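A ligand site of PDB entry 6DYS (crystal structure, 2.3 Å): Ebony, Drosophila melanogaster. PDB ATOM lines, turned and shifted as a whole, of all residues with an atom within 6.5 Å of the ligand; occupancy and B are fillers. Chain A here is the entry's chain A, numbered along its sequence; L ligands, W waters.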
ATOM      1  N   PHE A  25      24.444  -6.278  12.461  1.00  0.00           N
ATOM      2  CA  PHE A  25      25.650  -7.102  12.460  1.00  0.00           C
ATOM      3  C   PHE A  25      26.082  -7.570  13.842  1.00  0.00           C
ATOM      4  O   PHE A  25      26.474  -8.731  13.993  1.00  0.00           O
ATOM      5  CB  PHE A  25      26.807  -6.345  11.805  1.00  0.00           C
ATOM      6  CG  PHE A  25      26.767  -6.378  10.300  1.00  0.00           C
ATOM      7  CD1 PHE A  25      25.829  -5.617   9.609  1.00  0.00           C
ATOM      8  CD2 PHE A  25      27.645  -7.177   9.584  1.00  0.00           C
ATOM      9  CE1 PHE A  25      25.782  -5.648   8.235  1.00  0.00           C
ATOM     10  CE2 PHE A  25      27.598  -7.217   8.207  1.00  0.00           C
ATOM     11  CZ  PHE A  25      26.661  -6.451   7.528  1.00  0.00           C
ATOM     12  N   ALA A  29      25.898 -11.349  12.990  1.00  0.00           N
ATOM     13  CA  ALA A  29      26.672 -11.697  11.806  1.00  0.00           C
ATOM     14  C   ALA A  29      27.229 -13.107  11.937  1.00  0.00           C
ATOM     15  O   ALA A  29      27.787 -13.488  12.973  1.00  0.00           O
ATOM     16  CB  ALA A  29      27.790 -10.684  11.594  1.00  0.00           C
ATOM     17  N   ASP A  30      27.102 -13.886  10.854  1.00  0.00           N
ATOM     18  CA  ASP A  30      27.439 -15.302  10.897  1.00  0.00           C
ATOM     19  C   ASP A  30      28.946 -15.530  11.009  1.00  0.00           C
ATOM     20  O   ASP A  30      29.377 -16.573  11.508  1.00  0.00           O
ATOM     21  CB  ASP A  30      26.894 -16.028   9.660  1.00  0.00           C
ATOM     22  CG  ASP A  30      25.374 -15.904   9.539  1.00  0.00           C
ATOM     23  OD1 ASP A  30      24.882 -14.807   9.210  1.00  0.00           O
ATOM     24  OD2 ASP A  30      24.688 -16.916   9.741  1.00  0.00           O
ATOM     25  N   LEU A  31      29.763 -14.596  10.525  1.00  0.00           N
ATOM     26  CA  LEU A  31      31.204 -14.783  10.574  1.00  0.00           C
ATOM     27  C   LEU A  31      31.786 -14.362  11.921  1.00  0.00           C
ATOM     28  O   LEU A  31      32.517 -15.131  12.555  1.00  0.00           O
ATOM     29  CB  LEU A  31      31.888 -14.014   9.441  1.00  0.00           C
ATOM     30  CG  LEU A  31      31.748 -14.547   8.014  1.00  0.00           C
ATOM     31  CD1 LEU A  31      32.331 -13.540   7.030  1.00  0.00           C
ATOM     32  CD2 LEU A  31      32.437 -15.905   7.860  1.00  0.00           C
ATOM     33  N   GLU A  32      31.449 -13.153  12.370  1.00  0.00           N
ATOM     34  CA  GLU A  32      31.973 -12.631  13.634  1.00  0.00           C
ATOM     35  C   GLU A  32      31.597 -13.477  14.835  1.00  0.00           C
ATOM     36  O   GLU A  32      32.310 -13.416  15.850  1.00  0.00           O
ATOM     37  CB  GLU A  32      31.459 -11.211  13.903  1.00  0.00           C
ATOM     38  CG  GLU A  32      31.967 -10.164  12.965  1.00  0.00           C
ATOM     39  CD  GLU A  32      31.048  -9.973  11.781  1.00  0.00           C
ATOM     40  OE1 GLU A  32      30.985 -10.890  10.928  1.00  0.00           O
ATOM     41  OE2 GLU A  32      30.392  -8.916  11.712  1.00  0.00           O
ATOM     42  N   TYR A  44      32.027  -1.726  14.481  1.00  0.00           N
ATOM     43  CA  TYR A  44      31.279  -1.394  13.272  1.00  0.00           C
ATOM     44  C   TYR A  44      31.178   0.125  13.074  1.00  0.00           C
ATOM     45  O   TYR A  44      31.420   0.635  11.977  1.00  0.00           O
ATOM     46  CB  TYR A  44      29.887  -2.024  13.320  1.00  0.00           C
ATOM     47  CG  TYR A  44      29.901  -3.529  13.467  1.00  0.00           C
ATOM     48  CD1 TYR A  44      30.166  -4.350  12.381  1.00  0.00           C
ATOM     49  CD2 TYR A  44      29.652  -4.136  14.698  1.00  0.00           C
ATOM     50  CE1 TYR A  44      30.191  -5.731  12.513  1.00  0.00           C
ATOM     51  CE2 TYR A  44      29.669  -5.511  14.844  1.00  0.00           C
ATOM     52  CZ  TYR A  44      29.931  -6.302  13.738  1.00  0.00           C
ATOM     53  OH  TYR A  44      29.946  -7.670  13.866  1.00  0.00           O
ATOM     54  N   LEU A  93      37.495  -7.558  13.429  1.00  0.00           N
ATOM     55  CA  LEU A  93      36.825  -7.435  12.138  1.00  0.00           C
ATOM     56  C   LEU A  93      37.817  -7.424  10.969  1.00  0.00           C
ATOM     57  O   LEU A  93      37.410  -7.725   9.837  1.00  0.00           O
ATOM     58  CB  LEU A  93      35.992  -6.156  12.079  1.00  0.00           C
ATOM     59  CG  LEU A  93      34.717  -6.080  12.933  1.00  0.00           C
ATOM     60  CD1 LEU A  93      33.879  -4.868  12.555  1.00  0.00           C
ATOM     61  CD2 LEU A  93      33.918  -7.344  12.783  1.00  0.00           C
ATOM     62  N   VAL A  96      37.560 -10.640   9.367  1.00  0.00           N
ATOM     63  CA  VAL A  96      36.399 -10.719   8.488  1.00  0.00           C
ATOM     64  C   VAL A  96      36.696 -10.077   7.136  1.00  0.00           C
ATOM     65  O   VAL A  96      36.425 -10.655   6.084  1.00  0.00           O
ATOM     66  CB  VAL A  96      35.161 -10.084   9.152  1.00  0.00           C
ATOM     67  CG1 VAL A  96      34.031  -9.957   8.158  1.00  0.00           C
ATOM     68  CG2 VAL A  96      34.694 -10.922  10.345  1.00  0.00           C
ATOM     69  N   PHE A  97      37.289  -8.880   7.160  1.00  0.00           N
ATOM     70  CA  PHE A  97      37.536  -8.195   5.895  1.00  0.00           C
ATOM     71  C   PHE A  97      38.658  -8.845   5.096  1.00  0.00           C
ATOM     72  O   PHE A  97      38.606  -8.878   3.863  1.00  0.00           O
ATOM     73  CB  PHE A  97      37.805  -6.717   6.153  1.00  0.00           C
ATOM     74  CG  PHE A  97      36.570  -5.924   6.447  1.00  0.00           C
ATOM     75  CD1 PHE A  97      35.795  -5.406   5.424  1.00  0.00           C
ATOM     76  CD2 PHE A  97      36.150  -5.734   7.759  1.00  0.00           C
ATOM     77  CE1 PHE A  97      34.636  -4.692   5.690  1.00  0.00           C
ATOM     78  CE2 PHE A  97      34.993  -5.014   8.038  1.00  0.00           C
ATOM     79  CZ  PHE A  97      34.236  -4.493   7.003  1.00  0.00           C
ATOM     80  N   LEU A 100      36.946 -11.714   3.478  1.00  0.00           N
ATOM     81  CA  LEU A 100      36.138 -11.272   2.352  1.00  0.00           C
ATOM     82  C   LEU A 100      36.999 -10.936   1.144  1.00  0.00           C
ATOM     83  O   LEU A 100      36.633 -11.228   0.011  1.00  0.00           O
ATOM     84  CB  LEU A 100      35.283 -10.072   2.762  1.00  0.00           C
ATOM     85  CG  LEU A 100      34.217 -10.352   3.829  1.00  0.00           C
ATOM     86  CD1 LEU A 100      33.530  -9.063   4.291  1.00  0.00           C
ATOM     87  CD2 LEU A 100      33.182 -11.339   3.317  1.00  0.00           C
ATOM     88  N   GLU A 104      36.892 -12.345  -2.494  1.00  0.00           N
ATOM     89  CA  GLU A 104      36.566 -11.455  -3.596  1.00  0.00           C
ATOM     90  C   GLU A 104      37.764 -11.139  -4.478  1.00  0.00           C
ATOM     91  O   GLU A 104      37.613 -11.072  -5.703  1.00  0.00           O
ATOM     92  CB  GLU A 104      35.998 -10.138  -3.059  1.00  0.00           C
ATOM     93  CG  GLU A 104      34.634 -10.274  -2.445  1.00  0.00           C
ATOM     94  CD  GLU A 104      34.211  -9.028  -1.670  1.00  0.00           C
ATOM     95  OE1 GLU A 104      35.048  -8.112  -1.492  1.00  0.00           O
ATOM     96  OE2 GLU A 104      33.030  -8.978  -1.249  1.00  0.00           O
ATOM     97  N   SER A 122      28.353  -3.950  -3.507  1.00  0.00           N
ATOM     98  CA  SER A 122      27.373  -3.893  -2.431  1.00  0.00           C
ATOM     99  C   SER A 122      28.026  -4.543  -1.221  1.00  0.00           C
ATOM    100  O   SER A 122      27.995  -5.768  -1.065  1.00  0.00           O
ATOM    101  CB  SER A 122      26.072  -4.584  -2.839  1.00  0.00           C
ATOM    102  OG  SER A 122      25.183  -4.695  -1.732  1.00  0.00           O
ATOM    103  N   PHE A 123      28.633  -3.726  -0.356  1.00  0.00           N
ATOM    104  CA  PHE A 123      29.472  -4.291   0.696  1.00  0.00           C
ATOM    105  C   PHE A 123      28.791  -4.365   2.057  1.00  0.00           C
ATOM    106  O   PHE A 123      29.212  -5.155   2.897  1.00  0.00           O
ATOM    107  CB  PHE A 123      30.792  -3.504   0.806  1.00  0.00           C
ATOM    108  CG  PHE A 123      30.655  -2.134   1.418  1.00  0.00           C
ATOM    109  CD1 PHE A 123      30.932  -1.932   2.761  1.00  0.00           C
ATOM    110  CD2 PHE A 123      30.297  -1.041   0.650  1.00  0.00           C
ATOM    111  CE1 PHE A 123      30.830  -0.686   3.330  1.00  0.00           C
ATOM    112  CE2 PHE A 123      30.194   0.217   1.214  1.00  0.00           C
ATOM    113  CZ  PHE A 123      30.471   0.397   2.559  1.00  0.00           C
ATOM    114  N   MET A 124      27.752  -3.572   2.299  1.00  0.00           N
ATOM    115  CA  MET A 124      27.030  -3.654   3.553  1.00  0.00           C
ATOM    116  C   MET A 124      25.569  -3.340   3.297  1.00  0.00           C
ATOM    117  O   MET A 124      25.235  -2.442   2.502  1.00  0.00           O
ATOM    118  CB  MET A 124      27.589  -2.709   4.616  1.00  0.00           C
ATOM    119  CG  MET A 124      28.805  -3.271   5.338  1.00  0.00           C
ATOM    120  SD  MET A 124      28.945  -2.755   7.050  1.00  0.00           S
ATOM    121  CE  MET A 124      30.307  -1.601   6.936  1.00  0.00           C
ATOM    122  N   MET A 125      24.705  -4.088   3.970  1.00  0.00           N
ATOM    123  CA  MET A 125      23.262  -3.892   3.902  1.00  0.00           C
ATOM    124  C   MET A 125      22.723  -4.171   5.296  1.00  0.00           C
ATOM    125  O   MET A 125      23.217  -5.059   5.991  1.00  0.00           O
ATOM    126  CB  MET A 125      22.625  -4.809   2.858  1.00  0.00           C
ATOM    127  CG  MET A 125      21.367  -4.266   2.219  1.00  0.00           C
ATOM    128  SD  MET A 125      20.795  -5.308   0.858  1.00  0.00           S
ATOM    129  CE  MET A 125      21.370  -4.395  -0.564  1.00  0.00           C
ATOM    130  N   GLY A 126      21.722  -3.395   5.711  1.00  0.00           N
ATOM    131  CA  GLY A 126      21.147  -3.554   7.027  1.00  0.00           C
ATOM    132  C   GLY A 126      19.708  -3.095   7.055  1.00  0.00           C
ATOM    133  O   GLY A 126      19.270  -2.280   6.238  1.00  0.00           O
ATOM    134  N   MET A 140      14.339  -5.871   2.269  1.00  0.00           N
ATOM    135  CA  MET A 140      15.429  -6.515   1.540  1.00  0.00           C
ATOM    136  C   MET A 140      15.128  -6.559   0.046  1.00  0.00           C
ATOM    137  O   MET A 140      16.000  -6.237  -0.778  1.00  0.00           O
ATOM    138  CB  MET A 140      15.650  -7.916   2.099  1.00  0.00           C
ATOM    139  CG  MET A 140      16.252  -7.917   3.500  1.00  0.00           C
ATOM    140  SD  MET A 140      17.856  -7.080   3.526  1.00  0.00           S
ATOM    141  CE  MET A 140      18.897  -8.347   2.799  1.00  0.00           C
ATOM    142  N   GLU A 144      17.303  -4.483  -2.844  1.00  0.00           N
ATOM    143  CA  GLU A 144      17.812  -5.191  -4.005  1.00  0.00           C
ATOM    144  C   GLU A 144      17.343  -4.521  -5.291  1.00  0.00           C
ATOM    145  O   GLU A 144      18.146  -4.240  -6.190  1.00  0.00           O
ATOM    146  CB  GLU A 144      17.343  -6.644  -3.972  1.00  0.00           C
ATOM    147  CG  GLU A 144      17.884  -7.484  -5.104  1.00  0.00           C
ATOM    148  CD  GLU A 144      19.372  -7.286  -5.326  1.00  0.00           C
ATOM    149  OE1 GLU A 144      20.123  -7.231  -4.329  1.00  0.00           O
ATOM    150  OE2 GLU A 144      19.771  -7.173  -6.502  1.00  0.00           O
ATOM    151  N   THR A 161      29.014  -8.687  -4.702  1.00  0.00           N
ATOM    152  CA  THR A 161      28.804  -8.752  -3.266  1.00  0.00           C
ATOM    153  C   THR A 161      29.179 -10.146  -2.774  1.00  0.00           C
ATOM    154  O   THR A 161      29.155 -11.114  -3.532  1.00  0.00           O
ATOM    155  CB  THR A 161      27.350  -8.418  -2.897  1.00  0.00           C
ATOM    156  OG1 THR A 161      27.232  -8.208  -1.488  1.00  0.00           O
ATOM    157  CG2 THR A 161      26.394  -9.533  -3.317  1.00  0.00           C
ATOM    158  N   THR A 162      29.556 -10.223  -1.499  1.00  0.00           N
ATOM    159  CA  THR A 162      29.743 -11.495  -0.798  1.00  0.00           C
ATOM    160  C   THR A 162      28.646 -11.624   0.247  1.00  0.00           C
ATOM    161  O   THR A 162      28.554 -10.808   1.161  1.00  0.00           O
ATOM    162  CB  THR A 162      31.120 -11.579  -0.137  1.00  0.00           C
ATOM    163  OG1 THR A 162      32.114 -11.337  -1.126  1.00  0.00           O
ATOM    164  CG2 THR A 162      31.343 -12.964   0.439  1.00  0.00           C
ATOM    165  N   ASN A 163      27.810 -12.646   0.090  1.00  0.00           N
ATOM    166  CA  ASN A 163      26.710 -12.869   1.022  1.00  0.00           C
ATOM    167  C   ASN A 163      27.133 -13.939   2.019  1.00  0.00           C
ATOM    168  O   ASN A 163      27.579 -15.014   1.625  1.00  0.00           O
ATOM    169  CB  ASN A 163      25.437 -13.273   0.271  1.00  0.00           C
ATOM    170  CG  ASN A 163      24.846 -12.115  -0.521  1.00  0.00           C
ATOM    171  OD1 ASN A 163      24.667 -11.024   0.014  1.00  0.00           O
ATOM    172  ND2 ASN A 163      24.546 -12.346  -1.788  1.00  0.00           N
ATOM    173  N   THR A 164      26.993 -13.613   3.303  1.00  0.00           N
ATOM    174  CA  THR A 164      27.499 -14.448   4.377  1.00  0.00           C
ATOM    175  C   THR A 164      26.421 -14.997   5.282  1.00  0.00           C
ATOM    176  O   THR A 164      26.744 -15.710   6.239  1.00  0.00           O
ATOM    177  CB  THR A 164      28.524 -13.654   5.212  1.00  0.00           C
ATOM    178  OG1 THR A 164      27.910 -12.457   5.705  1.00  0.00           O
ATOM    179  CG2 THR A 164      29.726 -13.286   4.362  1.00  0.00           C
ATOM    180  N   THR A 168      20.544 -13.680   2.823  1.00  0.00           N
ATOM    181  CA  THR A 168      21.083 -12.879   1.738  1.00  0.00           C
ATOM    182  C   THR A 168      21.614 -13.751   0.605  1.00  0.00           C
ATOM    183  O   THR A 168      21.493 -13.393  -0.570  1.00  0.00           O
ATOM    184  CB  THR A 168      22.178 -11.941   2.257  1.00  0.00           C
ATOM    185  OG1 THR A 168      23.169 -12.691   2.969  1.00  0.00           O
ATOM    186  CG2 THR A 168      21.567 -10.884   3.181  1.00  0.00           C
HETATM  187  C1  LIG L   1      24.940  -8.306   1.457  1.00  0.00           C
HETATM  188  C2  LIG L   1      26.362  -8.046   1.927  1.00  0.00           C
HETATM  189  C3  LIG L   1      26.395  -7.465   3.384  1.00  0.00           C
HETATM  190  C4  LIG L   1      28.390  -8.930   3.987  1.00  0.00           C
HETATM  191  C5  LIG L   1      29.835  -8.336   4.157  1.00  0.00           C
HETATM  192  C6  LIG L   1      30.247  -8.228   5.557  1.00  0.00           C
HETATM  193  C7  LIG L   1      30.964  -7.097   5.997  1.00  0.00           C
HETATM  194  C8  LIG L   1      31.370  -6.986   7.334  1.00  0.00           C
HETATM  195  C9  LIG L   1      31.060  -7.987   8.238  1.00  0.00           C
HETATM  196  C10 LIG L   1      30.343  -9.118   7.798  1.00  0.00           C
HETATM  197  C11 LIG L   1      29.936  -9.226   6.452  1.00  0.00           C
HETATM  198  N1  LIG L   1      24.824  -8.219  -0.014  1.00  0.00           N
HETATM  199  N2  LIG L   1      27.398  -7.911   4.359  1.00  0.00           N
HETATM  200  O1  LIG L   1      25.615  -6.663   3.701  1.00  0.00           O
HETATM  201  O2  LIG L   1      31.480  -7.859   9.613  1.00  0.00           O
HETATM  202  O3  LIG L   1      29.988 -10.240   8.767  1.00  0.00           O
HETATM  203  O   HOH W   1      25.507 -11.061   3.361  1.00  0.00           O
HETATM  204  O   HOH W   2      23.189  -8.095   4.526  1.00  0.00           O
HETATM  205  O   HOH W   3      28.948 -12.422   8.736  1.00  0.00           O
HETATM  206  O   HOH W   4      29.502  -8.015   0.810  1.00  0.00           O
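ND2 of Asn 163 is in hydrogen-bond range of O of Thr 168 (3.4 Å).
The side-chain hydroxyl (OG1) of Thr 161 lies within hydrogen-bond range of the backbone carbonyl oxygen (O) of Ser 122 (2.6 Å).
The side-chain hydroxyl of Thr 162 is in hydrogen-bond range of the side-chain carboxylate of Glu 104 (2.5 Å).
OE2 of Glu 32 is in hydrogen-bond range of OH of Tyr 44, at 2.5 Å.
N of Met 125 sits at hydrogen-bond distance from O1 of the ligand (2.7 Å).
The side-chain hydroxyl (OG1) of Thr 161 lies within hydrogen-bond range of a nitrogen (N1) of the ligand, 2.8 Å away.
A nitrogen (N1) of the ligand sits at hydrogen-bond distance from the side-chain amide oxygen of Asn 163, at 2.8 Å.
O3 of the ligand is in hydrogen-bond range of OE1 of Glu 32 (2.5 Å).
Phe 25 touches the ligand.
CB of Ala 29 touches O3 of the ligand, at 3.6 Å.
Tyr 44 touches the ligand (CE1 to O2, 3.8 Å).
CG1 of Val 96 touches C9 of the ligand (3.6 Å).
Phe 97 touches the ligand.
CD1 of Leu 100 touches C6 of the ligand, 3.6 Å away.
Ser 122 touches the ligand (OG to N1, 3.9 Å).
O of Phe 123 touches C5 of the ligand, 3.5 Å away.
Met 124 touches the ligand.
Thr 162 touches the ligand.
Thr 164 touches the ligand.
Hydrophobic or aromatic side chains within 4 Å of the ligand: Phe 25, Ala 29, Tyr 44, Val 96, Phe 97, Leu 100 and Met 125.
Within 4 Å of the ligand: Phe 25, Ala 29, Glu 32, Tyr 44, Val 96, Phe 97, Leu 100, Ser 122, Phe 123, Met 124, Met 125, Thr 161, Thr 162, Asn 163 and Thr 164.
The nearest printed residue that does not touch the ligand is Leu 93 (4.03 Å).
Water W3 lies within hydrogen-bond range of an oxygen (O3) of the ligand (2.4 Å), the backbone NH (N) of Leu 31 (2.9 Å), the backbone NH (N) of Asp 30 (3.2 Å), the side-chain hydroxyl (OG1) of Thr 164 (3.2 Å) and the side-chain carboxylate (OE1) of Glu 32 (3.4 Å).
Water W2 lies within hydrogen-bond range of an oxygen (O1) of the ligand and the backbone carbonyl oxygen (O) of Met 125.
Water W4 lies within hydrogen-bond range of the backbone carbonyl oxygen of Thr 162 (3.0 Å), the side-chain hydroxyl of Thr 161 (3.2 Å) and the backbone carbonyl oxygen of Ser 122 (3.3 Å).
Water W1 lies within hydrogen-bond range of OG1 of Thr 168 (2.9 Å), N of Thr 164 (3.0 Å) and OD1 of Asn 163 (3.5 Å).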
